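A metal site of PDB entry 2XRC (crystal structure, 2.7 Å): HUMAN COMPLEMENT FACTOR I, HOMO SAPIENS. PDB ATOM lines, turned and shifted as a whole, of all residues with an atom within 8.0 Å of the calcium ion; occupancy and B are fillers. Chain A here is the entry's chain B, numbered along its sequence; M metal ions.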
ATOM      1  N   ARG A 169      41.178  13.277 -24.211  1.00  0.00           N
ATOM      2  CA  ARG A 169      39.927  12.959 -23.530  1.00  0.00           C
ATOM      3  C   ARG A 169      40.155  11.956 -22.397  1.00  0.00           C
ATOM      4  O   ARG A 169      39.541  12.074 -21.333  1.00  0.00           O
ATOM      5  CB  ARG A 169      38.903  12.409 -24.530  1.00  0.00           C
ATOM      6  CG  ARG A 169      37.593  11.965 -23.913  1.00  0.00           C
ATOM      7  CD  ARG A 169      36.608  11.545 -24.987  1.00  0.00           C
ATOM      8  NE  ARG A 169      35.406  10.932 -24.418  1.00  0.00           N
ATOM      9  CZ  ARG A 169      34.414  11.598 -23.831  1.00  0.00           C
ATOM     10  NH1 ARG A 169      34.454  12.929 -23.713  1.00  0.00           N
ATOM     11  NH2 ARG A 169      33.371  10.932 -23.348  1.00  0.00           N
ATOM     12  N   PHE A 246      29.779  16.036 -12.433  1.00  0.00           N
ATOM     13  CA  PHE A 246      28.339  16.064 -12.700  1.00  0.00           C
ATOM     14  C   PHE A 246      27.744  14.658 -12.596  1.00  0.00           C
ATOM     15  O   PHE A 246      28.155  13.762 -13.332  1.00  0.00           O
ATOM     16  CB  PHE A 246      28.089  16.641 -14.098  1.00  0.00           C
ATOM     17  CG  PHE A 246      26.639  16.676 -14.495  1.00  0.00           C
ATOM     18  CD1 PHE A 246      25.799  17.687 -14.045  1.00  0.00           C
ATOM     19  CD2 PHE A 246      26.115  15.701 -15.336  1.00  0.00           C
ATOM     20  CE1 PHE A 246      24.454  17.715 -14.422  1.00  0.00           C
ATOM     21  CE2 PHE A 246      24.773  15.725 -15.705  1.00  0.00           C
ATOM     22  CZ  PHE A 246      23.949  16.731 -15.250  1.00  0.00           C
ATOM     23  N   ILE A 254      30.984  12.582 -14.442  1.00  0.00           N
ATOM     24  CA  ILE A 254      31.736  12.998 -15.630  1.00  0.00           C
ATOM     25  C   ILE A 254      32.214  14.445 -15.451  1.00  0.00           C
ATOM     26  O   ILE A 254      31.714  15.147 -14.573  1.00  0.00           O
ATOM     27  CB  ILE A 254      30.881  12.864 -16.923  1.00  0.00           C
ATOM     28  CG1 ILE A 254      29.489  13.481 -16.743  1.00  0.00           C
ATOM     29  CG2 ILE A 254      30.741  11.401 -17.310  1.00  0.00           C
ATOM     30  CD1 ILE A 254      28.691  13.575 -18.031  1.00  0.00           C
ATOM     31  N   PRO A 255      33.178  14.896 -16.266  1.00  0.00           N
ATOM     32  CA  PRO A 255      33.627  16.291 -16.190  1.00  0.00           C
ATOM     33  C   PRO A 255      32.476  17.289 -16.342  1.00  0.00           C
ATOM     34  O   PRO A 255      31.563  17.075 -17.141  1.00  0.00           O
ATOM     35  CB  PRO A 255      34.614  16.418 -17.357  1.00  0.00           C
ATOM     36  CG  PRO A 255      35.140  15.053 -17.553  1.00  0.00           C
ATOM     37  CD  PRO A 255      34.017  14.115 -17.210  1.00  0.00           C
ATOM     38  N   SER A 256      32.523  18.373 -15.569  1.00  0.00           N
ATOM     39  CA  SER A 256      31.459  19.380 -15.577  1.00  0.00           C
ATOM     40  C   SER A 256      31.368  20.133 -16.901  1.00  0.00           C
ATOM     41  O   SER A 256      30.272  20.479 -17.334  1.00  0.00           O
ATOM     42  CB  SER A 256      31.638  20.369 -14.424  1.00  0.00           C
ATOM     43  OG  SER A 256      31.414  19.722 -13.178  1.00  0.00           O
ATOM     44  N   GLN A 257      32.515  20.392 -17.538  1.00  0.00           N
ATOM     45  CA  GLN A 257      32.539  21.126 -18.818  1.00  0.00           C
ATOM     46  C   GLN A 257      31.857  20.336 -19.949  1.00  0.00           C
ATOM     47  O   GLN A 257      31.363  20.932 -20.910  1.00  0.00           O
ATOM     48  CB  GLN A 257      33.972  21.532 -19.219  1.00  0.00           C
ATOM     49  CG  GLN A 257      34.886  20.416 -19.725  1.00  0.00           C
ATOM     50  CD  GLN A 257      35.599  19.661 -18.619  1.00  0.00           C
ATOM     51  OE1 GLN A 257      35.189  19.693 -17.455  1.00  0.00           O
ATOM     52  NE2 GLN A 257      36.682  18.968 -18.977  1.00  0.00           N
ATOM     53  N   TYR A 258      31.820  19.014 -19.817  1.00  0.00           N
ATOM     54  CA  TYR A 258      31.112  18.150 -20.777  1.00  0.00           C
ATOM     55  C   TYR A 258      29.597  18.413 -20.823  1.00  0.00           C
ATOM     56  O   TYR A 258      28.920  17.935 -21.728  1.00  0.00           O
ATOM     57  CB  TYR A 258      31.342  16.675 -20.456  1.00  0.00           C
ATOM     58  CG  TYR A 258      32.716  16.109 -20.802  1.00  0.00           C
ATOM     59  CD1 TYR A 258      33.739  16.922 -21.298  1.00  0.00           C
ATOM     60  CD2 TYR A 258      32.989  14.773 -20.586  1.00  0.00           C
ATOM     61  CE1 TYR A 258      34.989  16.393 -21.599  1.00  0.00           C
ATOM     62  CE2 TYR A 258      34.234  14.234 -20.878  1.00  0.00           C
ATOM     63  CZ  TYR A 258      35.230  15.049 -21.387  1.00  0.00           C
ATOM     64  OH  TYR A 258      36.462  14.512 -21.674  1.00  0.00           O
ATOM     65  N   GLN A 259      29.067  19.128 -19.827  1.00  0.00           N
ATOM     66  CA  GLN A 259      27.702  19.643 -19.889  1.00  0.00           C
ATOM     67  C   GLN A 259      27.566  20.603 -21.070  1.00  0.00           C
ATOM     68  O   GLN A 259      28.458  21.404 -21.324  1.00  0.00           O
ATOM     69  CB  GLN A 259      27.337  20.385 -18.599  1.00  0.00           C
ATOM     70  CG  GLN A 259      27.152  19.495 -17.385  1.00  0.00           C
ATOM     71  CD  GLN A 259      26.586  20.253 -16.192  1.00  0.00           C
ATOM     72  OE1 GLN A 259      25.397  20.186 -15.903  1.00  0.00           O
ATOM     73  NE2 GLN A 259      27.450  20.991 -15.491  1.00  0.00           N
ATOM     74  N   CYS A 260      26.444  20.511 -21.772  1.00  0.00           N
ATOM     75  CA  CYS A 260      26.193  21.321 -22.975  1.00  0.00           C
ATOM     76  C   CYS A 260      27.426  21.449 -23.852  1.00  0.00           C
ATOM     77  O   CYS A 260      27.908  22.560 -24.093  1.00  0.00           O
ATOM     78  CB  CYS A 260      25.706  22.728 -22.584  1.00  0.00           C
ATOM     79  SG  CYS A 260      24.217  22.788 -21.592  1.00  0.00           S
ATOM     80  N   ASN A 261      27.959  20.315 -24.318  1.00  0.00           N
ATOM     81  CA  ASN A 261      29.098  20.331 -25.253  1.00  0.00           C
ATOM     82  C   ASN A 261      28.792  19.692 -26.618  1.00  0.00           C
ATOM     83  O   ASN A 261      29.700  19.488 -27.418  1.00  0.00           O
ATOM     84  CB  ASN A 261      30.344  19.703 -24.623  1.00  0.00           C
ATOM     85  CG  ASN A 261      30.312  18.182 -24.606  1.00  0.00           C
ATOM     86  OD1 ASN A 261      29.240  17.560 -24.659  1.00  0.00           O
ATOM     87  ND2 ASN A 261      31.481  17.563 -24.510  1.00  0.00           N
ATOM     88  N   GLY A 262      27.517  19.375 -26.853  1.00  0.00           N
ATOM     89  CA  GLY A 262      27.077  18.790 -28.128  1.00  0.00           C
ATOM     90  C   GLY A 262      26.923  17.285 -28.076  1.00  0.00           C
ATOM     91  O   GLY A 262      25.898  16.750 -28.494  1.00  0.00           O
ATOM     92  N   GLU A 263      27.953  16.607 -27.563  1.00  0.00           N
ATOM     93  CA  GLU A 263      27.913  15.154 -27.403  1.00  0.00           C
ATOM     94  C   GLU A 263      27.183  14.764 -26.123  1.00  0.00           C
ATOM     95  O   GLU A 263      27.330  15.417 -25.084  1.00  0.00           O
ATOM     96  CB  GLU A 263      29.341  14.586 -27.361  1.00  0.00           C
ATOM     97  CG  GLU A 263      29.396  13.063 -27.352  1.00  0.00           C
ATOM     98  CD  GLU A 263      30.785  12.507 -27.112  1.00  0.00           C
ATOM     99  OE1 GLU A 263      30.888  11.330 -26.708  1.00  0.00           O
ATOM    100  OE2 GLU A 263      31.790  13.240 -27.330  1.00  0.00           O
ATOM    101  N   VAL A 264      26.388  13.692 -26.202  1.00  0.00           N
ATOM    102  CA  VAL A 264      25.704  13.128 -25.052  1.00  0.00           C
ATOM    103  C   VAL A 264      26.630  12.127 -24.364  1.00  0.00           C
ATOM    104  O   VAL A 264      27.148  11.224 -25.014  1.00  0.00           O
ATOM    105  CB  VAL A 264      24.404  12.393 -25.459  1.00  0.00           C
ATOM    106  CG1 VAL A 264      23.641  11.909 -24.240  1.00  0.00           C
ATOM    107  CG2 VAL A 264      23.519  13.295 -26.313  1.00  0.00           C
ATOM    108  N   ASP A 265      26.844  12.310 -23.052  1.00  0.00           N
ATOM    109  CA  ASP A 265      27.721  11.432 -22.265  1.00  0.00           C
ATOM    110  C   ASP A 265      26.960  10.523 -21.308  1.00  0.00           C
ATOM    111  O   ASP A 265      27.316   9.359 -21.141  1.00  0.00           O
ATOM    112  CB  ASP A 265      28.703  12.253 -21.435  1.00  0.00           C
ATOM    113  CG  ASP A 265      29.489  13.255 -22.273  1.00  0.00           C
ATOM    114  OD1 ASP A 265      29.505  13.149 -23.517  1.00  0.00           O
ATOM    115  OD2 ASP A 265      30.087  14.150 -21.658  1.00  0.00           O
ATOM    116  N   CYS A 266      25.936  11.066 -20.647  1.00  0.00           N
ATOM    117  CA  CYS A 266      25.071  10.260 -19.772  1.00  0.00           C
ATOM    118  C   CYS A 266      24.128   9.435 -20.639  1.00  0.00           C
ATOM    119  O   CYS A 266      23.517   9.956 -21.568  1.00  0.00           O
ATOM    120  CB  CYS A 266      24.233  11.141 -18.833  1.00  0.00           C
ATOM    121  SG  CYS A 266      25.079  12.538 -18.042  1.00  0.00           S
ATOM    122  N   GLY A 269      21.016  11.097 -20.707  1.00  0.00           N
ATOM    123  CA  GLY A 269      21.060  12.194 -21.689  1.00  0.00           C
ATOM    124  C   GLY A 269      20.660  13.572 -21.179  1.00  0.00           C
ATOM    125  O   GLY A 269      20.304  14.447 -21.972  1.00  0.00           O
ATOM    126  N   GLU A 270      20.749  13.775 -19.863  1.00  0.00           N
ATOM    127  CA  GLU A 270      20.280  15.018 -19.239  1.00  0.00           C
ATOM    128  C   GLU A 270      21.388  16.055 -19.064  1.00  0.00           C
ATOM    129  O   GLU A 270      21.152  17.126 -18.496  1.00  0.00           O
ATOM    130  CB  GLU A 270      19.574  14.716 -17.897  1.00  0.00           C
ATOM    131  CG  GLU A 270      20.481  14.519 -16.675  1.00  0.00           C
ATOM    132  CD  GLU A 270      21.183  13.177 -16.672  1.00  0.00           C
ATOM    133  OE1 GLU A 270      21.754  12.795 -17.715  1.00  0.00           O
ATOM    134  OE2 GLU A 270      21.174  12.513 -15.617  1.00  0.00           O
ATOM    135  N   ASP A 271      22.595  15.746 -19.543  1.00  0.00           N
ATOM    136  CA  ASP A 271      23.679  16.737 -19.582  1.00  0.00           C
ATOM    137  C   ASP A 271      23.608  17.586 -20.863  1.00  0.00           C
ATOM    138  O   ASP A 271      24.388  18.530 -21.011  1.00  0.00           O
ATOM    139  CB  ASP A 271      25.052  16.062 -19.453  1.00  0.00           C
ATOM    140  CG  ASP A 271      25.495  15.366 -20.727  1.00  0.00           C
ATOM    141  OD1 ASP A 271      24.649  14.823 -21.456  1.00  0.00           O
ATOM    142  OD2 ASP A 271      26.718  15.369 -21.007  1.00  0.00           O
ATOM    143  N   GLU A 272      22.707  17.228 -21.769  1.00  0.00           N
ATOM    144  CA  GLU A 272      22.411  18.050 -22.953  1.00  0.00           C
ATOM    145  C   GLU A 272      20.948  18.498 -22.975  1.00  0.00           C
ATOM    146  O   GLU A 272      20.412  18.806 -24.049  1.00  0.00           O
ATOM    147  CB  GLU A 272      22.744  17.302 -24.245  1.00  0.00           C
ATOM    148  CG  GLU A 272      24.199  16.873 -24.371  1.00  0.00           C
ATOM    149  CD  GLU A 272      25.161  18.051 -24.383  1.00  0.00           C
ATOM    150  OE1 GLU A 272      26.082  18.071 -23.530  1.00  0.00           O
ATOM    151  OE2 GLU A 272      25.001  18.942 -25.245  1.00  0.00           O
ATOM    152  N   VAL A 273      20.302  18.530 -21.811  1.00  0.00           N
ATOM    153  CA  VAL A 273      18.921  19.024 -21.729  1.00  0.00           C
ATOM    154  C   VAL A 273      18.925  20.459 -21.229  1.00  0.00           C
ATOM    155  O   VAL A 273      19.546  20.782 -20.210  1.00  0.00           O
ATOM    156  CB  VAL A 273      18.026  18.141 -20.829  1.00  0.00           C
ATOM    157  CG1 VAL A 273      18.453  18.227 -19.368  1.00  0.00           C
ATOM    158  CG2 VAL A 273      16.571  18.554 -21.004  1.00  0.00           C
ATOM    159  N   CYS A 275      20.078  23.484 -23.199  1.00  0.00           N
ATOM    160  CA  CYS A 275      21.368  24.090 -23.551  1.00  0.00           C
ATOM    161  C   CYS A 275      21.223  25.151 -24.643  1.00  0.00           C
ATOM    162  O   CYS A 275      21.747  26.258 -24.528  1.00  0.00           O
ATOM    163  CB  CYS A 275      22.374  23.021 -23.989  1.00  0.00           C
ATOM    164  SG  CYS A 275      22.815  21.834 -22.697  1.00  0.00           S
ATOM    165  N   ARG A 298      33.680  12.630 -32.728  1.00  0.00           N
ATOM    166  CA  ARG A 298      32.347  13.201 -32.518  1.00  0.00           C
ATOM    167  C   ARG A 298      31.579  13.356 -33.825  1.00  0.00           C
ATOM    168  O   ARG A 298      30.363  13.189 -33.862  1.00  0.00           O
ATOM    169  CB  ARG A 298      32.446  14.567 -31.830  1.00  0.00           C
ATOM    170  CG  ARG A 298      32.807  14.488 -30.356  1.00  0.00           C
ATOM    171  CD  ARG A 298      32.829  15.872 -29.714  1.00  0.00           C
ATOM    172  NE  ARG A 298      31.575  16.602 -29.906  1.00  0.00           N
ATOM    173  CZ  ARG A 298      31.347  17.842 -29.487  1.00  0.00           C
ATOM    174  NH1 ARG A 298      32.272  18.526 -28.829  1.00  0.00           N
ATOM    175  NH2 ARG A 298      30.163  18.403 -29.726  1.00  0.00           N
HETATM  176 CA    CA M   1      27.789  16.383 -22.871  1.00  0.00          CA
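OH of Tyr 258 sits close to NH1 of Arg 169 (3.3 Å). The backbone NH of Cys 260 sits at hydrogen-bond distance from the backbone carbonyl oxygen of Asp 271 (3.0 Å). OE1 of Glu 272 lies close to N of Cys 260, at 3.0 Å. The backbone NH of Gly 262 lies within hydrogen-bond range of the side-chain carboxylate of Glu 272, at 3.0 Å. The backbone carbonyl oxygen (O) of Asn 261 sits at hydrogen-bond distance from the guanidinium group (NH2) of Arg 298 (2.6 Å). SG of Cys 260 forms a disulfide with SG of Cys 275 (2.0 Å).
Merely in contact with the calcium ion: Asp 265. Six residues have an atom within 4 Å of the calcium ion: Tyr 258, Asn 261, Glu 263, Asp 265, Asp 271 and Glu 272.
The backbone carbonyl oxygen (O) of Tyr 258 is bound to the calcium ion, 2.2 Å away. OD2 of Asp 271 is bound to the calcium ion (2.4 Å). The calcium ion is bound by O of Glu 263, 2.5 Å away. OE1 of Glu 272 binds the calcium ion. The calcium ion is bound by the side-chain amide oxygen (OD1) of Asn 261.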
